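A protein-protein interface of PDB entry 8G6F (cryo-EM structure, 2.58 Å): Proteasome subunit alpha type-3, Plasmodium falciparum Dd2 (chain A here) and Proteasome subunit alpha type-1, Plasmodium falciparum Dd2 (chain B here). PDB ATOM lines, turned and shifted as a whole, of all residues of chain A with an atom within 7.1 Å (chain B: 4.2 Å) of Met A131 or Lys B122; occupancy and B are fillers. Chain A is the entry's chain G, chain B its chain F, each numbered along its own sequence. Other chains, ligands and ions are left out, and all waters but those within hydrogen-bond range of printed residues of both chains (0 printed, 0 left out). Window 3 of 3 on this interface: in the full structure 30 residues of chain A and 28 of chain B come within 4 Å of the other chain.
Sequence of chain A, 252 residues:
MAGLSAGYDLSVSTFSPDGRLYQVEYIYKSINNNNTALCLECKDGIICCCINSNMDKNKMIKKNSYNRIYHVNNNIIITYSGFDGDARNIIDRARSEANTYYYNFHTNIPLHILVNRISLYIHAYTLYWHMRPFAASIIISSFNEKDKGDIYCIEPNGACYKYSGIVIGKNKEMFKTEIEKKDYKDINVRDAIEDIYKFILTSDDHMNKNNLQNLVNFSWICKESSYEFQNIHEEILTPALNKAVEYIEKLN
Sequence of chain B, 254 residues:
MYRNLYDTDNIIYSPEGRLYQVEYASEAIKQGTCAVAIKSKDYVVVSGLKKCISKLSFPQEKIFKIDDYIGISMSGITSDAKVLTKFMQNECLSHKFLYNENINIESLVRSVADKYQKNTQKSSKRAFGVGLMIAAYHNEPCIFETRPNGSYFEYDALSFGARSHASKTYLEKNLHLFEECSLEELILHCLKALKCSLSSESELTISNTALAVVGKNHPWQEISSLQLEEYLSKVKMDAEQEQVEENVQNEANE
Hydrophobic or aromatic side chains of chain B within 4 Å of the printed part of chain A: Ile B11.
Hydrophobic or aromatic side chains of chain A within 4 Å of the printed part of chain B: Tyr A125, His A130 and Met A131.
ND2 of Asn B10 sits at hydrogen-bond distance from O of Lys B122, at 2.8 Å.
The side-chain amide nitrogen (ND2) of Asn B10 is in hydrogen-bond range of the backbone carbonyl oxygen (O) of Lys B125, at 3.1 Å.
A ring nitrogen (NE2) of His A130 lies close to the side-chain sulfur of Met A131 (3.6 Å).
Among the printed residues, merely in contact across the chains: Tyr A125 with Gln B121 (3.1 Å), Trp A129 with Ile B11 (3.7 Å), His A130 with Ile B11 (3.9 Å), His A130 with Lys B122 (3.7 Å), Met A131 with Gln B121 (3.4 Å), Met A131 with Lys B122 (3.7 Å), Arg A132 with Asn B10 (3.7 Å) and Arg A132 with Ile B11 (3.8 Å).
Printed residues of chain B within 4 Å of His A130: Ile B11, Lys B122 and Ser B123.
Met A131 touches just these residues of chain B: Gln B121 (3.4 Å) and Lys B122 (3.7 Å).
Of the printed residues of chain A, Asn B10 touches Arg A132.
Of the printed residues of chain A, Thr B120 touches Arg A132 (2.8 Å).
Of the printed residues of chain A, Lys B122 touches His A130 and Met A131.
The nearest residue of chain B that does not touch Met A131 is Ile B11 (4.1 Å).
The backbone NH (N) of Ser B123 lies within hydrogen-bond range of the backbone carbonyl oxygen (O) of His A130 (3.3 Å).
The backbone carbonyl oxygen of Gln B121 lies within hydrogen-bond range of the backbone NH of Arg A132 (2.9 Å).
The guanidinium group (NE) of Arg A132 sits at hydrogen-bond distance from the backbone carbonyl oxygen (O) of Thr B120 (2.8 Å).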
ATOM      1  N   VAL A  12      11.232  19.583  -3.755  1.00  0.00           N
ATOM      2  CA  VAL A  12      12.640  19.564  -4.133  1.00  0.00           C
ATOM      3  C   VAL A  12      12.842  19.632  -5.637  1.00  0.00           C
ATOM      4  O   VAL A  12      13.972  19.870  -6.087  1.00  0.00           O
ATOM      5  CB  VAL A  12      13.338  18.304  -3.584  1.00  0.00           C
ATOM      6  CG1 VAL A  12      13.056  17.103  -4.469  1.00  0.00           C
ATOM      7  CG2 VAL A  12      14.829  18.537  -3.459  1.00  0.00           C
ATOM      8  N   ALA A 124      20.298  11.417  -6.754  1.00  0.00           N
ATOM      9  CA  ALA A 124      19.098  10.897  -7.399  1.00  0.00           C
ATOM     10  C   ALA A 124      17.838  11.212  -6.607  1.00  0.00           C
ATOM     11  O   ALA A 124      16.747  11.272  -7.183  1.00  0.00           O
ATOM     12  CB  ALA A 124      19.223   9.389  -7.597  1.00  0.00           C
ATOM     13  N   TYR A 125      17.953  11.411  -5.299  1.00  0.00           N
ATOM     14  CA  TYR A 125      16.782  11.661  -4.468  1.00  0.00           C
ATOM     15  C   TYR A 125      16.378  13.125  -4.429  1.00  0.00           C
ATOM     16  O   TYR A 125      15.358  13.450  -3.816  1.00  0.00           O
ATOM     17  CB  TYR A 125      17.033  11.156  -3.047  1.00  0.00           C
ATOM     18  CG  TYR A 125      16.819   9.674  -2.910  1.00  0.00           C
ATOM     19  CD1 TYR A 125      17.735   8.774  -3.425  1.00  0.00           C
ATOM     20  CD2 TYR A 125      15.693   9.173  -2.280  1.00  0.00           C
ATOM     21  CE1 TYR A 125      17.540   7.419  -3.310  1.00  0.00           C
ATOM     22  CE2 TYR A 125      15.491   7.816  -2.159  1.00  0.00           C
ATOM     23  CZ  TYR A 125      16.417   6.945  -2.677  1.00  0.00           C
ATOM     24  OH  TYR A 125      16.221   5.590  -2.560  1.00  0.00           O
ATOM     25  N   THR A 126      17.138  14.010  -5.070  1.00  0.00           N
ATOM     26  CA  THR A 126      16.806  15.423  -5.160  1.00  0.00           C
ATOM     27  C   THR A 126      16.157  15.780  -6.490  1.00  0.00           C
ATOM     28  O   THR A 126      16.104  16.959  -6.849  1.00  0.00           O
ATOM     29  CB  THR A 126      18.058  16.274  -4.950  1.00  0.00           C
ATOM     30  OG1 THR A 126      19.009  15.999  -5.984  1.00  0.00           O
ATOM     31  CG2 THR A 126      18.688  15.980  -3.609  1.00  0.00           C
ATOM     32  N   LEU A 127      15.654  14.788  -7.227  1.00  0.00           N
ATOM     33  CA  LEU A 127      15.170  15.008  -8.581  1.00  0.00           C
ATOM     34  C   LEU A 127      13.667  14.836  -8.749  1.00  0.00           C
ATOM     35  O   LEU A 127      13.111  15.392  -9.697  1.00  0.00           O
ATOM     36  CB  LEU A 127      15.878  14.054  -9.554  1.00  0.00           C
ATOM     37  CG  LEU A 127      17.352  14.351  -9.828  1.00  0.00           C
ATOM     38  CD1 LEU A 127      18.024  13.147 -10.447  1.00  0.00           C
ATOM     39  CD2 LEU A 127      17.500  15.564 -10.724  1.00  0.00           C
ATOM     40  N   TYR A 128      13.001  14.099  -7.868  1.00  0.00           N
ATOM     41  CA  TYR A 128      11.602  13.747  -8.047  1.00  0.00           C
ATOM     42  C   TYR A 128      10.741  14.387  -6.968  1.00  0.00           C
ATOM     43  O   TYR A 128      11.219  14.747  -5.890  1.00  0.00           O
ATOM     44  CB  TYR A 128      11.419  12.228  -8.027  1.00  0.00           C
ATOM     45  CG  TYR A 128      12.431  11.502  -8.871  1.00  0.00           C
ATOM     46  CD1 TYR A 128      12.286  11.428 -10.244  1.00  0.00           C
ATOM     47  CD2 TYR A 128      13.540  10.904  -8.297  1.00  0.00           C
ATOM     48  CE1 TYR A 128      13.210  10.774 -11.022  1.00  0.00           C
ATOM     49  CE2 TYR A 128      14.471  10.247  -9.065  1.00  0.00           C
ATOM     50  CZ  TYR A 128      14.302  10.184 -10.428  1.00  0.00           C
ATOM     51  OH  TYR A 128      15.227   9.529 -11.201  1.00  0.00           O
ATOM     52  N   TRP A 129       9.453  14.511  -7.273  1.00  0.00           N
ATOM     53  CA  TRP A 129       8.503  15.193  -6.408  1.00  0.00           C
ATOM     54  C   TRP A 129       7.818  14.259  -5.420  1.00  0.00           C
ATOM     55  O   TRP A 129       6.875  14.680  -4.744  1.00  0.00           O
ATOM     56  CB  TRP A 129       7.453  15.925  -7.254  1.00  0.00           C
ATOM     57  CG  TRP A 129       6.530  15.046  -8.056  1.00  0.00           C
ATOM     58  CD1 TRP A 129       6.502  13.682  -8.088  1.00  0.00           C
ATOM     59  CD2 TRP A 129       5.495  15.485  -8.941  1.00  0.00           C
ATOM     60  NE1 TRP A 129       5.517  13.248  -8.934  1.00  0.00           N
ATOM     61  CE2 TRP A 129       4.884  14.336  -9.473  1.00  0.00           C
ATOM     62  CE3 TRP A 129       5.028  16.740  -9.338  1.00  0.00           C
ATOM     63  CZ2 TRP A 129       3.833  14.402 -10.378  1.00  0.00           C
ATOM     64  CZ3 TRP A 129       3.984  16.803 -10.234  1.00  0.00           C
ATOM     65  CH2 TRP A 129       3.398  15.642 -10.745  1.00  0.00           C
ATOM     66  N   HIS A 130       8.263  13.005  -5.323  1.00  0.00           N
ATOM     67  CA  HIS A 130       7.634  12.029  -4.444  1.00  0.00           C
ATOM     68  C   HIS A 130       8.622  11.353  -3.501  1.00  0.00           C
ATOM     69  O   HIS A 130       8.226  10.448  -2.763  1.00  0.00           O
ATOM     70  CB  HIS A 130       6.899  10.969  -5.270  1.00  0.00           C
ATOM     71  CG  HIS A 130       7.808  10.088  -6.067  1.00  0.00           C
ATOM     72  ND1 HIS A 130       8.559  10.554  -7.123  1.00  0.00           N
ATOM     73  CD2 HIS A 130       8.086   8.768  -5.963  1.00  0.00           C
ATOM     74  CE1 HIS A 130       9.262   9.561  -7.634  1.00  0.00           C
ATOM     75  NE2 HIS A 130       8.992   8.465  -6.949  1.00  0.00           N
ATOM     76  N   MET A 131       9.885  11.765  -3.497  1.00  0.00           N
ATOM     77  CA  MET A 131      10.900  11.190  -2.629  1.00  0.00           C
ATOM     78  C   MET A 131      11.481  12.273  -1.732  1.00  0.00           C
ATOM     79  O   MET A 131      11.516  13.450  -2.096  1.00  0.00           O
ATOM     80  CB  MET A 131      12.026  10.534  -3.436  1.00  0.00           C
ATOM     81  CG  MET A 131      11.559   9.533  -4.477  1.00  0.00           C
ATOM     82  SD  MET A 131      10.664   8.134  -3.777  1.00  0.00           S
ATOM     83  CE  MET A 131      11.923   7.382  -2.753  1.00  0.00           C
ATOM     84  N   ARG A 132      11.930  11.862  -0.547  1.00  0.00           N
ATOM     85  CA  ARG A 132      12.542  12.775   0.404  1.00  0.00           C
ATOM     86  C   ARG A 132      14.052  12.726   0.256  1.00  0.00           C
ATOM     87  O   ARG A 132      14.634  11.636   0.371  1.00  0.00           O
ATOM     88  CB  ARG A 132      12.147  12.412   1.829  1.00  0.00           C
ATOM     89  CG  ARG A 132      12.753  13.321   2.879  1.00  0.00           C
ATOM     90  CD  ARG A 132      12.286  12.962   4.271  1.00  0.00           C
ATOM     91  NE  ARG A 132      12.741  11.643   4.686  1.00  0.00           N
ATOM     92  CZ  ARG A 132      13.932  11.384   5.206  1.00  0.00           C
ATOM     93  NH1 ARG A 132      14.834  12.334   5.377  1.00  0.00           N
ATOM     94  NH2 ARG A 132      14.228  10.137   5.559  1.00  0.00           N
ATOM     95  N   PRO A 133      14.729  13.845   0.005  1.00  0.00           N
ATOM     96  CA  PRO A 133      16.194  13.813  -0.072  1.00  0.00           C
ATOM     97  C   PRO A 133      16.830  13.411   1.252  1.00  0.00           C
ATOM     98  O   PRO A 133      16.280  13.641   2.329  1.00  0.00           O
ATOM     99  CB  PRO A 133      16.561  15.251  -0.448  1.00  0.00           C
ATOM    100  CG  PRO A 133      15.340  15.832  -1.014  1.00  0.00           C
ATOM    101  CD  PRO A 133      14.194  15.171  -0.343  1.00  0.00           C
ATOM    102  N   ASN B  10       5.146  14.066   4.455  1.00  0.00           N
ATOM    103  CA  ASN B  10       6.287  13.546   5.193  1.00  0.00           C
ATOM    104  C   ASN B  10       7.606  13.667   4.445  1.00  0.00           C
ATOM    105  O   ASN B  10       8.630  13.206   4.958  1.00  0.00           O
ATOM    106  CB  ASN B  10       6.045  12.080   5.561  1.00  0.00           C
ATOM    107  CG  ASN B  10       5.880  11.196   4.348  1.00  0.00           C
ATOM    108  OD1 ASN B  10       5.421  11.643   3.299  1.00  0.00           O
ATOM    109  ND2 ASN B  10       6.251   9.929   4.484  1.00  0.00           N
ATOM    110  N   ILE B  11       7.620  14.267   3.257  1.00  0.00           N
ATOM    111  CA  ILE B  11       8.844  14.422   2.483  1.00  0.00           C
ATOM    112  C   ILE B  11       9.283  15.876   2.406  1.00  0.00           C
ATOM    113  O   ILE B  11      10.191  16.204   1.636  1.00  0.00           O
ATOM    114  CB  ILE B  11       8.698  13.824   1.074  1.00  0.00           C
ATOM    115  CG1 ILE B  11       7.573  14.516   0.306  1.00  0.00           C
ATOM    116  CG2 ILE B  11       8.439  12.331   1.155  1.00  0.00           C
ATOM    117  CD1 ILE B  11       7.635  14.297  -1.177  1.00  0.00           C
ATOM    118  N   THR B 120       9.781   6.502   5.718  1.00  0.00           N
ATOM    119  CA  THR B 120       9.849   7.953   5.826  1.00  0.00           C
ATOM    120  C   THR B 120      10.394   8.623   4.573  1.00  0.00           C
ATOM    121  O   THR B 120      10.541   9.846   4.561  1.00  0.00           O
ATOM    122  CB  THR B 120      10.712   8.352   7.025  1.00  0.00           C
ATOM    123  OG1 THR B 120      12.066   7.945   6.800  1.00  0.00           O
ATOM    124  CG2 THR B 120      10.200   7.703   8.291  1.00  0.00           C
ATOM    125  N   GLN B 121      10.690   7.860   3.521  1.00  0.00           N
ATOM    126  CA  GLN B 121      11.319   8.405   2.327  1.00  0.00           C
ATOM    127  C   GLN B 121      10.351   8.635   1.176  1.00  0.00           C
ATOM    128  O   GLN B 121      10.705   9.343   0.229  1.00  0.00           O
ATOM    129  CB  GLN B 121      12.439   7.473   1.851  1.00  0.00           C
ATOM    130  CG  GLN B 121      13.755   7.644   2.592  1.00  0.00           C
ATOM    131  CD  GLN B 121      14.708   8.599   1.897  1.00  0.00           C
ATOM    132  OE1 GLN B 121      14.728   8.694   0.672  1.00  0.00           O
ATOM    133  NE2 GLN B 121      15.505   9.313   2.679  1.00  0.00           N
ATOM    134  N   LYS B 122       9.151   8.065   1.226  1.00  0.00           N
ATOM    135  CA  LYS B 122       8.168   8.201   0.163  1.00  0.00           C
ATOM    136  C   LYS B 122       6.948   8.955   0.671  1.00  0.00           C
ATOM    137  O   LYS B 122       6.610   8.893   1.856  1.00  0.00           O
ATOM    138  CB  LYS B 122       7.733   6.836  -0.372  1.00  0.00           C
ATOM    139  CG  LYS B 122       8.770   6.154  -1.238  1.00  0.00           C
ATOM    140  CD  LYS B 122       8.149   5.594  -2.509  1.00  0.00           C
ATOM    141  CE  LYS B 122       8.922   4.393  -3.038  1.00  0.00           C
ATOM    142  NZ  LYS B 122       8.084   3.163  -3.057  1.00  0.00           N
ATOM    143  N   SER B 123       6.287   9.670  -0.239  1.00  0.00           N
ATOM    144  CA  SER B 123       5.083  10.410   0.109  1.00  0.00           C
ATOM    145  C   SER B 123       3.841   9.535   0.150  1.00  0.00           C
ATOM    146  O   SER B 123       2.807   9.979   0.656  1.00  0.00           O
ATOM    147  CB  SER B 123       4.860  11.552  -0.882  1.00  0.00           C
ATOM    148  OG  SER B 123       4.726  11.060  -2.200  1.00  0.00           O
ATOM    149  N   SER B 124       3.915   8.311  -0.363  1.00  0.00           N
ATOM    150  CA  SER B 124       2.794   7.384  -0.338  1.00  0.00           C
ATOM    151  C   SER B 124       2.759   6.540   0.924  1.00  0.00           C
ATOM    152  O   SER B 124       1.898   5.664   1.044  1.00  0.00           O
ATOM    153  CB  SER B 124       2.847   6.469  -1.561  1.00  0.00           C
ATOM    154  OG  SER B 124       4.066   5.753  -1.604  1.00  0.00           O
ATOM    155  N   LYS B 125       3.671   6.779   1.862  1.00  0.00           N
ATOM    156  CA  LYS B 125       3.782   6.007   3.087  1.00  0.00           C
ATOM    157  C   LYS B 125       3.801   6.961   4.272  1.00  0.00           C
ATOM    158  O   LYS B 125       3.686   8.179   4.119  1.00  0.00           O
ATOM    159  CB  LYS B 125       5.038   5.129   3.060  1.00  0.00           C
ATOM    160  CG  LYS B 125       5.011   4.084   1.967  1.00  0.00           C
ATOM    161  CD  LYS B 125       6.250   3.224   1.988  1.00  0.00           C
ATOM    162  CE  LYS B 125       5.998   1.888   1.312  1.00  0.00           C
ATOM    163  NZ  LYS B 125       5.211   0.959   2.172  1.00  0.00           N
